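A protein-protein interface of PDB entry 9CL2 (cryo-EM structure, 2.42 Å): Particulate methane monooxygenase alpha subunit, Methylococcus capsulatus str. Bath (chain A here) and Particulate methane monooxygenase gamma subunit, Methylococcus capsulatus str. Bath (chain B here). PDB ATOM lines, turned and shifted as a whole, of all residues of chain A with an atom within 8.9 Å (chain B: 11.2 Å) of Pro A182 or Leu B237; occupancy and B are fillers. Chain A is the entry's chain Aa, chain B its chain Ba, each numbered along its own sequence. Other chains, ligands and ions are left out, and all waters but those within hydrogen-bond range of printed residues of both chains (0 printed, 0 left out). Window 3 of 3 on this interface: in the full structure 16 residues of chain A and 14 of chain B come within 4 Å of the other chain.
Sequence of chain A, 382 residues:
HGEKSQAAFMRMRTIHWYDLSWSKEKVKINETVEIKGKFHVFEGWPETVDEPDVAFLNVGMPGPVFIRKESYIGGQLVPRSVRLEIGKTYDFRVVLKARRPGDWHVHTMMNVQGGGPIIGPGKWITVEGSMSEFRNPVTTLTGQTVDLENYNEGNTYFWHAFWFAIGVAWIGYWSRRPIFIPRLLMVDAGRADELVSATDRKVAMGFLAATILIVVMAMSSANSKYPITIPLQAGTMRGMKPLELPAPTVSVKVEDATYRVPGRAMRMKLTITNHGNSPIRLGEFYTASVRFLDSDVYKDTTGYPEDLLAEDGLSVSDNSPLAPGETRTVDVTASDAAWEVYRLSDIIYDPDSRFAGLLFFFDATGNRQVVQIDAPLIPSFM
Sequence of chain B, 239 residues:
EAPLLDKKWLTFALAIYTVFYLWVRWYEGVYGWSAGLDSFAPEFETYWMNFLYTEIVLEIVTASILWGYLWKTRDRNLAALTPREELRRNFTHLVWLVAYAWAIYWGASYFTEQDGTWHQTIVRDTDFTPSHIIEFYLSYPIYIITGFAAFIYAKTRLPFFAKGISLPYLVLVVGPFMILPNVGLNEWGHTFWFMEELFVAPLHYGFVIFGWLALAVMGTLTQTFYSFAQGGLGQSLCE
OH of Tyr B226 lies within hydrogen-bond range of OD2 of Asp A188, at 2.7 Å.
Phe A180 touches Phe B225 (CB to CZ, 3.4 Å).
Phe B225 touches Ile A181 (CD1 to CG1, 3.96 Å).
Phe B228 touches Ile A181.
Ile A181 touches Leu B237 (CG2 to CD2, 3.7 Å).
Pro A182 touches Leu B237 (CG to CD2, 3.6 Å).
Of the printed residues of chain B, Pro A182 touches Leu B237 (3.6 Å).
Leu B237 touches two residues of chain A.
Pro A178 touches none of the printed residues of chain B.
Ile A181 touches just these residues of chain B: Phe B225 (3.96 Å), Phe B228 (3.98 Å) and Leu B237 (3.7 Å).
No residue of chain A comes within 4 Å of Ser B236.
Of the printed residues of chain A, Phe B225 touches Phe A180 (3.4 Å) and Ile A181 (3.96 Å).
Of the printed residues of chain B, Asp A188 touches Tyr B226.
Printed residues of chain A within 4 Å of Phe B228: Ile A181.
Of the printed residues of chain A, Tyr B226 touches Asp A188 (2.7 Å).
Phe B91 touches none of the printed residues of chain A.
The nearest residue of chain B that does not touch Pro A182 is Cys B238 (6.8 Å).
The nearest printed residue of chain A that does not touch Tyr B226 is Leu A184 (4.2 Å).
Printed residues of chain A that touch a printed residue of chain B: Phe A180, Ile A181, Pro A182 and Asp A188.
Of the 17 printed residues of chain B, 4 touch a printed residue of chain A.
Among the printed residues, no Asp or Glu carboxylate lies within 4 Å of a Lys or Arg side-chain nitrogen of the other chain.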
ATOM      1  N   ARG A 177     -13.657  29.986 -11.105  1.00  0.00           N
ATOM      2  CA  ARG A 177     -14.504  30.312  -9.973  1.00  0.00           C
ATOM      3  C   ARG A 177     -14.989  29.044  -9.283  1.00  0.00           C
ATOM      4  O   ARG A 177     -14.819  27.936  -9.801  1.00  0.00           O
ATOM      5  CB  ARG A 177     -15.703  31.145 -10.442  1.00  0.00           C
ATOM      6  CG  ARG A 177     -15.335  32.512 -10.987  1.00  0.00           C
ATOM      7  CD  ARG A 177     -16.512  33.149 -11.703  1.00  0.00           C
ATOM      8  NE  ARG A 177     -16.332  33.159 -13.149  1.00  0.00           N
ATOM      9  CZ  ARG A 177     -17.190  33.693 -14.008  1.00  0.00           C
ATOM     10  NH1 ARG A 177     -18.307  34.270 -13.598  1.00  0.00           N
ATOM     11  NH2 ARG A 177     -16.920  33.644 -15.309  1.00  0.00           N
ATOM     12  N   PRO A 178     -15.575  29.167  -8.091  1.00  0.00           N
ATOM     13  CA  PRO A 178     -16.246  28.009  -7.487  1.00  0.00           C
ATOM     14  C   PRO A 178     -17.284  27.436  -8.439  1.00  0.00           C
ATOM     15  O   PRO A 178     -18.016  28.170  -9.106  1.00  0.00           O
ATOM     16  CB  PRO A 178     -16.897  28.584  -6.222  1.00  0.00           C
ATOM     17  CG  PRO A 178     -16.387  29.991  -6.075  1.00  0.00           C
ATOM     18  CD  PRO A 178     -15.357  30.252  -7.121  1.00  0.00           C
ATOM     19  N   ILE A 179     -17.340  26.108  -8.501  1.00  0.00           N
ATOM     20  CA  ILE A 179     -18.021  25.396  -9.579  1.00  0.00           C
ATOM     21  C   ILE A 179     -19.358  24.818  -9.123  1.00  0.00           C
ATOM     22  O   ILE A 179     -20.410  25.176  -9.654  1.00  0.00           O
ATOM     23  CB  ILE A 179     -17.114  24.297 -10.175  1.00  0.00           C
ATOM     24  CG1 ILE A 179     -15.807  24.902 -10.691  1.00  0.00           C
ATOM     25  CG2 ILE A 179     -17.839  23.550 -11.281  1.00  0.00           C
ATOM     26  CD1 ILE A 179     -14.879  23.895 -11.333  1.00  0.00           C
ATOM     27  N   PHE A 180     -19.339  23.915  -8.144  1.00  0.00           N
ATOM     28  CA  PHE A 180     -20.478  23.038  -7.903  1.00  0.00           C
ATOM     29  C   PHE A 180     -21.289  23.413  -6.669  1.00  0.00           C
ATOM     30  O   PHE A 180     -22.482  23.702  -6.786  1.00  0.00           O
ATOM     31  CB  PHE A 180     -19.987  21.590  -7.795  1.00  0.00           C
ATOM     32  CG  PHE A 180     -19.611  20.980  -9.113  1.00  0.00           C
ATOM     33  CD1 PHE A 180     -20.547  20.852 -10.127  1.00  0.00           C
ATOM     34  CD2 PHE A 180     -18.321  20.531  -9.341  1.00  0.00           C
ATOM     35  CE1 PHE A 180     -20.202  20.290 -11.340  1.00  0.00           C
ATOM     36  CE2 PHE A 180     -17.971  19.967 -10.552  1.00  0.00           C
ATOM     37  CZ  PHE A 180     -18.912  19.847 -11.553  1.00  0.00           C
ATOM     38  N   ILE A 181     -20.681  23.426  -5.487  1.00  0.00           N
ATOM     39  CA  ILE A 181     -21.453  23.546  -4.251  1.00  0.00           C
ATOM     40  C   ILE A 181     -21.933  24.979  -4.031  1.00  0.00           C
ATOM     41  O   ILE A 181     -23.142  25.182  -3.833  1.00  0.00           O
ATOM     42  CB  ILE A 181     -20.654  23.026  -3.042  1.00  0.00           C
ATOM     43  CG1 ILE A 181     -20.669  21.496  -3.017  1.00  0.00           C
ATOM     44  CG2 ILE A 181     -21.230  23.572  -1.746  1.00  0.00           C
ATOM     45  CD1 ILE A 181     -20.136  20.896  -1.734  1.00  0.00           C
ATOM     46  N   PRO A 182     -21.059  26.001  -4.033  1.00  0.00           N
ATOM     47  CA  PRO A 182     -21.574  27.364  -3.805  1.00  0.00           C
ATOM     48  C   PRO A 182     -22.576  27.808  -4.856  1.00  0.00           C
ATOM     49  O   PRO A 182     -23.566  28.468  -4.521  1.00  0.00           O
ATOM     50  CB  PRO A 182     -20.309  28.238  -3.823  1.00  0.00           C
ATOM     51  CG  PRO A 182     -19.162  27.311  -3.747  1.00  0.00           C
ATOM     52  CD  PRO A 182     -19.607  26.002  -4.287  1.00  0.00           C
ATOM     53  N   ARG A 183     -22.350  27.450  -6.122  1.00  0.00           N
ATOM     54  CA  ARG A 183     -23.297  27.814  -7.170  1.00  0.00           C
ATOM     55  C   ARG A 183     -24.633  27.110  -6.976  1.00  0.00           C
ATOM     56  O   ARG A 183     -25.694  27.714  -7.177  1.00  0.00           O
ATOM     57  CB  ARG A 183     -22.706  27.496  -8.543  1.00  0.00           C
ATOM     58  CG  ARG A 183     -21.626  28.471  -8.983  1.00  0.00           C
ATOM     59  CD  ARG A 183     -21.143  28.181 -10.394  1.00  0.00           C
ATOM     60  NE  ARG A 183     -22.017  28.755 -11.409  1.00  0.00           N
ATOM     61  CZ  ARG A 183     -21.862  29.962 -11.933  1.00  0.00           C
ATOM     62  NH1 ARG A 183     -20.880  30.761 -11.550  1.00  0.00           N
ATOM     63  NH2 ARG A 183     -22.714  30.379 -12.865  1.00  0.00           N
ATOM     64  N   LEU A 184     -24.603  25.834  -6.585  1.00  0.00           N
ATOM     65  CA  LEU A 184     -25.842  25.113  -6.310  1.00  0.00           C
ATOM     66  C   LEU A 184     -26.608  25.754  -5.161  1.00  0.00           C
ATOM     67  O   LEU A 184     -27.833  25.913  -5.233  1.00  0.00           O
ATOM     68  CB  LEU A 184     -25.538  23.648  -5.996  1.00  0.00           C
ATOM     69  CG  LEU A 184     -26.707  22.759  -5.567  1.00  0.00           C
ATOM     70  CD1 LEU A 184     -27.564  22.376  -6.763  1.00  0.00           C
ATOM     71  CD2 LEU A 184     -26.195  21.519  -4.852  1.00  0.00           C
ATOM     72  N   LEU A 185     -25.902  26.129  -4.090  1.00  0.00           N
ATOM     73  CA  LEU A 185     -26.568  26.780  -2.966  1.00  0.00           C
ATOM     74  C   LEU A 185     -27.148  28.130  -3.370  1.00  0.00           C
ATOM     75  O   LEU A 185     -28.256  28.485  -2.950  1.00  0.00           O
ATOM     76  CB  LEU A 185     -25.597  26.938  -1.796  1.00  0.00           C
ATOM     77  CG  LEU A 185     -24.998  25.646  -1.238  1.00  0.00           C
ATOM     78  CD1 LEU A 185     -23.947  25.953  -0.184  1.00  0.00           C
ATOM     79  CD2 LEU A 185     -26.086  24.747  -0.672  1.00  0.00           C
ATOM     80  N   MET A 186     -26.416  28.900  -4.180  1.00  0.00           N
ATOM     81  CA  MET A 186     -26.920  30.195  -4.623  1.00  0.00           C
ATOM     82  C   MET A 186     -28.155  30.041  -5.503  1.00  0.00           C
ATOM     83  O   MET A 186     -29.110  30.818  -5.384  1.00  0.00           O
ATOM     84  CB  MET A 186     -25.822  30.961  -5.363  1.00  0.00           C
ATOM     85  CG  MET A 186     -24.710  31.469  -4.461  1.00  0.00           C
ATOM     86  SD  MET A 186     -24.997  33.149  -3.874  1.00  0.00           S
ATOM     87  CE  MET A 186     -24.760  34.081  -5.385  1.00  0.00           C
ATOM     88  N   VAL A 187     -28.153  29.051  -6.398  1.00  0.00           N
ATOM     89  CA  VAL A 187     -29.328  28.806  -7.233  1.00  0.00           C
ATOM     90  C   VAL A 187     -30.509  28.376  -6.374  1.00  0.00           C
ATOM     91  O   VAL A 187     -31.644  28.822  -6.584  1.00  0.00           O
ATOM     92  CB  VAL A 187     -29.007  27.766  -8.323  1.00  0.00           C
ATOM     93  CG1 VAL A 187     -30.273  27.358  -9.058  1.00  0.00           C
ATOM     94  CG2 VAL A 187     -27.992  28.324  -9.302  1.00  0.00           C
ATOM     95  N   ASP A 188     -30.265  27.504  -5.393  1.00  0.00           N
ATOM     96  CA  ASP A 188     -31.335  27.082  -4.494  1.00  0.00           C
ATOM     97  C   ASP A 188     -31.862  28.255  -3.674  1.00  0.00           C
ATOM     98  O   ASP A 188     -33.065  28.347  -3.410  1.00  0.00           O
ATOM     99  CB  ASP A 188     -30.843  25.964  -3.577  1.00  0.00           C
ATOM    100  CG  ASP A 188     -30.658  24.650  -4.309  1.00  0.00           C
ATOM    101  OD1 ASP A 188     -31.211  24.504  -5.419  1.00  0.00           O
ATOM    102  OD2 ASP A 188     -29.962  23.763  -3.774  1.00  0.00           O
ATOM    103  N   ALA A 189     -30.974  29.159  -3.263  1.00  0.00           N
ATOM    104  CA  ALA A 189     -31.363  30.324  -2.479  1.00  0.00           C
ATOM    105  C   ALA A 189     -32.068  31.392  -3.305  1.00  0.00           C
ATOM    106  O   ALA A 189     -32.581  32.357  -2.729  1.00  0.00           O
ATOM    107  CB  ALA A 189     -30.135  30.933  -1.796  1.00  0.00           C
ATOM    108  N   ARG A 191     -30.504  33.172  -5.824  1.00  0.00           N
ATOM    109  CA  ARG A 191     -29.529  34.149  -6.292  1.00  0.00           C
ATOM    110  C   ARG A 191     -28.858  33.720  -7.592  1.00  0.00           C
ATOM    111  O   ARG A 191     -27.668  33.986  -7.792  1.00  0.00           O
ATOM    112  CB  ARG A 191     -28.480  34.405  -5.210  1.00  0.00           C
ATOM    113  CG  ARG A 191     -29.060  34.826  -3.871  1.00  0.00           C
ATOM    114  CD  ARG A 191     -28.179  35.862  -3.193  1.00  0.00           C
ATOM    115  NE  ARG A 191     -27.439  35.295  -2.072  1.00  0.00           N
ATOM    116  CZ  ARG A 191     -26.350  35.836  -1.542  1.00  0.00           C
ATOM    117  NH1 ARG A 191     -25.842  36.964  -2.011  1.00  0.00           N
ATOM    118  NH2 ARG A 191     -25.757  35.229  -0.520  1.00  0.00           N
ATOM    119  N   ALA A 192     -29.600  33.051  -8.478  1.00  0.00           N
ATOM    120  CA  ALA A 192     -29.020  32.584  -9.733  1.00  0.00           C
ATOM    121  C   ALA A 192     -28.587  33.740 -10.624  1.00  0.00           C
ATOM    122  O   ALA A 192     -27.545  33.653 -11.286  1.00  0.00           O
ATOM    123  CB  ALA A 192     -30.016  31.691 -10.471  1.00  0.00           C
ATOM    124  N   LEU A 195     -25.009  34.907 -10.590  1.00  0.00           N
ATOM    125  CA  LEU A 195     -23.933  34.031 -11.032  1.00  0.00           C
ATOM    126  C   LEU A 195     -23.435  34.352 -12.435  1.00  0.00           C
ATOM    127  O   LEU A 195     -22.375  33.849 -12.824  1.00  0.00           O
ATOM    128  CB  LEU A 195     -24.389  32.571 -10.969  1.00  0.00           C
ATOM    129  CG  LEU A 195     -24.650  32.018  -9.568  1.00  0.00           C
ATOM    130  CD1 LEU A 195     -25.151  30.588  -9.641  1.00  0.00           C
ATOM    131  CD2 LEU A 195     -23.398  32.108  -8.712  1.00  0.00           C
ATOM    132  N   LEU B  87     -17.935  14.216   7.132  1.00  0.00           N
ATOM    133  CA  LEU B  87     -17.256  14.840   6.000  1.00  0.00           C
ATOM    134  C   LEU B  87     -16.136  13.952   5.470  1.00  0.00           C
ATOM    135  O   LEU B  87     -15.934  13.846   4.253  1.00  0.00           O
ATOM    136  CB  LEU B  87     -16.716  16.210   6.409  1.00  0.00           C
ATOM    137  CG  LEU B  87     -15.994  17.035   5.343  1.00  0.00           C
ATOM    138  CD1 LEU B  87     -16.925  17.351   4.187  1.00  0.00           C
ATOM    139  CD2 LEU B  87     -15.447  18.313   5.953  1.00  0.00           C
ATOM    140  N   PHE B  91     -15.813  12.358   1.739  1.00  0.00           N
ATOM    141  CA  PHE B  91     -14.632  12.392   0.880  1.00  0.00           C
ATOM    142  C   PHE B  91     -14.241  10.992   0.418  1.00  0.00           C
ATOM    143  O   PHE B  91     -13.845  10.799  -0.738  1.00  0.00           O
ATOM    144  CB  PHE B  91     -13.468  13.064   1.606  1.00  0.00           C
ATOM    145  CG  PHE B  91     -13.354  14.535   1.332  1.00  0.00           C
ATOM    146  CD1 PHE B  91     -13.101  14.993   0.050  1.00  0.00           C
ATOM    147  CD2 PHE B  91     -13.498  15.459   2.352  1.00  0.00           C
ATOM    148  CE1 PHE B  91     -12.994  16.344  -0.209  1.00  0.00           C
ATOM    149  CE2 PHE B  91     -13.393  16.813   2.099  1.00  0.00           C
ATOM    150  CZ  PHE B  91     -13.141  17.256   0.816  1.00  0.00           C
ATOM    151  N   THR B 222     -25.928  15.387  -7.350  1.00  0.00           N
ATOM    152  CA  THR B 222     -26.659  16.355  -6.542  1.00  0.00           C
ATOM    153  C   THR B 222     -26.800  15.848  -5.116  1.00  0.00           C
ATOM    154  O   THR B 222     -26.434  16.544  -4.158  1.00  0.00           O
ATOM    155  CB  THR B 222     -28.030  16.631  -7.160  1.00  0.00           C
ATOM    156  OG1 THR B 222     -27.881  16.890  -8.561  1.00  0.00           O
ATOM    157  CG2 THR B 222     -28.671  17.838  -6.501  1.00  0.00           C
ATOM    158  N   PHE B 225     -23.618  16.135  -3.250  1.00  0.00           N
ATOM    159  CA  PHE B 225     -23.325  17.493  -2.812  1.00  0.00           C
ATOM    160  C   PHE B 225     -24.113  17.836  -1.558  1.00  0.00           C
ATOM    161  O   PHE B 225     -23.572  18.431  -0.618  1.00  0.00           O
ATOM    162  CB  PHE B 225     -23.619  18.487  -3.933  1.00  0.00           C
ATOM    163  CG  PHE B 225     -22.635  18.425  -5.061  1.00  0.00           C
ATOM    164  CD1 PHE B 225     -21.326  18.037  -4.831  1.00  0.00           C
ATOM    165  CD2 PHE B 225     -23.013  18.756  -6.349  1.00  0.00           C
ATOM    166  CE1 PHE B 225     -20.415  17.976  -5.864  1.00  0.00           C
ATOM    167  CE2 PHE B 225     -22.107  18.699  -7.386  1.00  0.00           C
ATOM    168  CZ  PHE B 225     -20.805  18.307  -7.143  1.00  0.00           C
ATOM    169  N   TYR B 226     -25.385  17.431  -1.507  1.00  0.00           N
ATOM    170  CA  TYR B 226     -26.166  17.670  -0.303  1.00  0.00           C
ATOM    171  C   TYR B 226     -25.584  16.901   0.874  1.00  0.00           C
ATOM    172  O   TYR B 226     -25.508  17.427   1.992  1.00  0.00           O
ATOM    173  CB  TYR B 226     -27.628  17.299  -0.540  1.00  0.00           C
ATOM    174  CG  TYR B 226     -28.360  18.316  -1.384  1.00  0.00           C
ATOM    175  CD1 TYR B 226     -28.279  19.672  -1.092  1.00  0.00           C
ATOM    176  CD2 TYR B 226     -29.122  17.927  -2.475  1.00  0.00           C
ATOM    177  CE1 TYR B 226     -28.940  20.609  -1.859  1.00  0.00           C
ATOM    178  CE2 TYR B 226     -29.788  18.859  -3.249  1.00  0.00           C
ATOM    179  CZ  TYR B 226     -29.692  20.198  -2.936  1.00  0.00           C
ATOM    180  OH  TYR B 226     -30.353  21.127  -3.704  1.00  0.00           O
ATOM    181  N   PHE B 228     -22.577  16.413   1.266  1.00  0.00           N
ATOM    182  CA  PHE B 228     -21.418  17.204   1.654  1.00  0.00           C
ATOM    183  C   PHE B 228     -21.814  18.463   2.414  1.00  0.00           C
ATOM    184  O   PHE B 228     -21.023  18.968   3.219  1.00  0.00           O
ATOM    185  CB  PHE B 228     -20.604  17.579   0.414  1.00  0.00           C
ATOM    186  CG  PHE B 228     -19.427  16.681   0.165  1.00  0.00           C
ATOM    187  CD1 PHE B 228     -18.313  16.731   0.984  1.00  0.00           C
ATOM    188  CD2 PHE B 228     -19.432  15.793  -0.897  1.00  0.00           C
ATOM    189  CE1 PHE B 228     -17.227  15.909   0.752  1.00  0.00           C
ATOM    190  CE2 PHE B 228     -18.351  14.968  -1.133  1.00  0.00           C
ATOM    191  CZ  PHE B 228     -17.246  15.026  -0.308  1.00  0.00           C
ATOM    192  N   ALA B 229     -23.021  18.983   2.181  1.00  0.00           N
ATOM    193  CA  ALA B 229     -23.377  20.307   2.676  1.00  0.00           C
ATOM    194  C   ALA B 229     -24.256  20.281   3.918  1.00  0.00           C
ATOM    195  O   ALA B 229     -24.255  21.252   4.683  1.00  0.00           O
ATOM    196  CB  ALA B 229     -24.081  21.105   1.575  1.00  0.00           C
ATOM    197  N   GLN B 230     -25.010  19.203   4.138  1.00  0.00           N
ATOM    198  CA  GLN B 230     -25.937  19.159   5.263  1.00  0.00           C
ATOM    199  C   GLN B 230     -25.238  19.089   6.615  1.00  0.00           C
ATOM    200  O   GLN B 230     -25.892  19.310   7.639  1.00  0.00           O
ATOM    201  CB  GLN B 230     -26.886  17.968   5.115  1.00  0.00           C
ATOM    202  CG  GLN B 230     -26.222  16.617   5.310  1.00  0.00           C
ATOM    203  CD  GLN B 230     -27.226  15.507   5.547  1.00  0.00           C
ATOM    204  OE1 GLN B 230     -28.388  15.611   5.155  1.00  0.00           O
ATOM    205  NE2 GLN B 230     -26.781  14.435   6.192  1.00  0.00           N
ATOM    206  N   GLY B 231     -23.939  18.796   6.644  1.00  0.00           N
ATOM    207  CA  GLY B 231     -23.198  18.666   7.880  1.00  0.00           C
ATOM    208  C   GLY B 231     -22.658  19.950   8.461  1.00  0.00           C
ATOM    209  O   GLY B 231     -21.932  19.909   9.457  1.00  0.00           O
ATOM    210  N   GLY B 232     -22.990  21.097   7.873  1.00  0.00           N
ATOM    211  CA  GLY B 232     -22.492  22.376   8.327  1.00  0.00           C
ATOM    212  C   GLY B 232     -21.480  23.025   7.408  1.00  0.00           C
ATOM    213  O   GLY B 232     -21.152  24.201   7.609  1.00  0.00           O
ATOM    214  N   LEU B 233     -20.972  22.294   6.413  1.00  0.00           N
ATOM    215  CA  LEU B 233     -20.054  22.893   5.449  1.00  0.00           C
ATOM    216  C   LEU B 233     -20.748  23.971   4.627  1.00  0.00           C
ATOM    217  O   LEU B 233     -20.160  25.021   4.344  1.00  0.00           O
ATOM    218  CB  LEU B 233     -19.471  21.811   4.539  1.00  0.00           C
ATOM    219  CG  LEU B 233     -18.774  22.288   3.263  1.00  0.00           C
ATOM    220  CD1 LEU B 233     -17.317  22.618   3.541  1.00  0.00           C
ATOM    221  CD2 LEU B 233     -18.891  21.247   2.161  1.00  0.00           C
ATOM    222  N   GLY B 234     -22.000  23.727   4.233  1.00  0.00           N
ATOM    223  CA  GLY B 234     -22.719  24.702   3.429  1.00  0.00           C
ATOM    224  C   GLY B 234     -22.951  26.014   4.154  1.00  0.00           C
ATOM    225  O   GLY B 234     -22.838  27.089   3.561  1.00  0.00           O
ATOM    226  N   GLN B 235     -23.288  25.944   5.444  1.00  0.00           N
ATOM    227  CA  GLN B 235     -23.523  27.164   6.212  1.00  0.00           C
ATOM    228  C   GLN B 235     -22.257  28.004   6.323  1.00  0.00           C
ATOM    229  O   GLN B 235     -22.303  29.231   6.177  1.00  0.00           O
ATOM    230  CB  GLN B 235     -24.058  26.814   7.602  1.00  0.00           C
ATOM    231  CG  GLN B 235     -25.053  27.821   8.162  1.00  0.00           C
ATOM    232  CD  GLN B 235     -26.203  28.108   7.215  1.00  0.00           C
ATOM    233  OE1 GLN B 235     -26.593  29.260   7.028  1.00  0.00           O
ATOM    234  NE2 GLN B 235     -26.761  27.058   6.624  1.00  0.00           N
ATOM    235  N   SER B 236     -21.116  27.362   6.583  1.00  0.00           N
ATOM    236  CA  SER B 236     -19.858  28.095   6.663  1.00  0.00           C
ATOM    237  C   SER B 236     -19.449  28.644   5.302  1.00  0.00           C
ATOM    238  O   SER B 236     -18.911  29.753   5.210  1.00  0.00           O
ATOM    239  CB  SER B 236     -18.761  27.195   7.230  1.00  0.00           C
ATOM    240  OG  SER B 236     -19.124  26.688   8.502  1.00  0.00           O
ATOM    241  N   LEU B 237     -19.695  27.880   4.236  1.00  0.00           N
ATOM    242  CA  LEU B 237     -19.304  28.320   2.901  1.00  0.00           C
ATOM    243  C   LEU B 237     -20.161  29.481   2.411  1.00  0.00           C
ATOM    244  O   LEU B 237     -19.663  30.359   1.699  1.00  0.00           O
ATOM    245  CB  LEU B 237     -19.386  27.146   1.925  1.00  0.00           C
ATOM    246  CG  LEU B 237     -18.740  27.337   0.554  1.00  0.00           C
ATOM    247  CD1 LEU B 237     -17.238  27.512   0.688  1.00  0.00           C
ATOM    248  CD2 LEU B 237     -19.063  26.152  -0.334  1.00  0.00           C
ATOM    249  N   CYS B 238     -21.446  29.503   2.776  1.00  0.00           N
ATOM    250  CA  CYS B 238     -22.330  30.577   2.339  1.00  0.00           C
ATOM    251  C   CYS B 238     -21.974  31.916   2.971  1.00  0.00           C
ATOM    252  O   CYS B 238     -22.347  32.961   2.428  1.00  0.00           O
ATOM    253  CB  CYS B 238     -23.783  30.220   2.655  1.00  0.00           C
ATOM    254  SG  CYS B 238     -25.010  31.295   1.874  1.00  0.00           S
ATOM    255  N   GLU B 239     -21.267  31.910   4.097  1.00  0.00           N
ATOM    256  CA  GLU B 239     -20.874  33.147   4.763  1.00  0.00           C
ATOM    257  C   GLU B 239     -19.839  33.909   3.944  1.00  0.00           C
ATOM    258  O   GLU B 239     -19.652  35.112   4.126  1.00  0.00           O
ATOM    259  CB  GLU B 239     -20.324  32.850   6.160  1.00  0.00           C
ATOM    260  CG  GLU B 239     -21.354  32.292   7.127  1.00  0.00           C
ATOM    261  CD  GLU B 239     -20.779  32.043   8.508  1.00  0.00           C
ATOM    262  OE1 GLU B 239     -19.556  32.225   8.686  1.00  0.00           O
ATOM    263  OE2 GLU B 239     -21.549  31.665   9.415  1.00  0.00           O
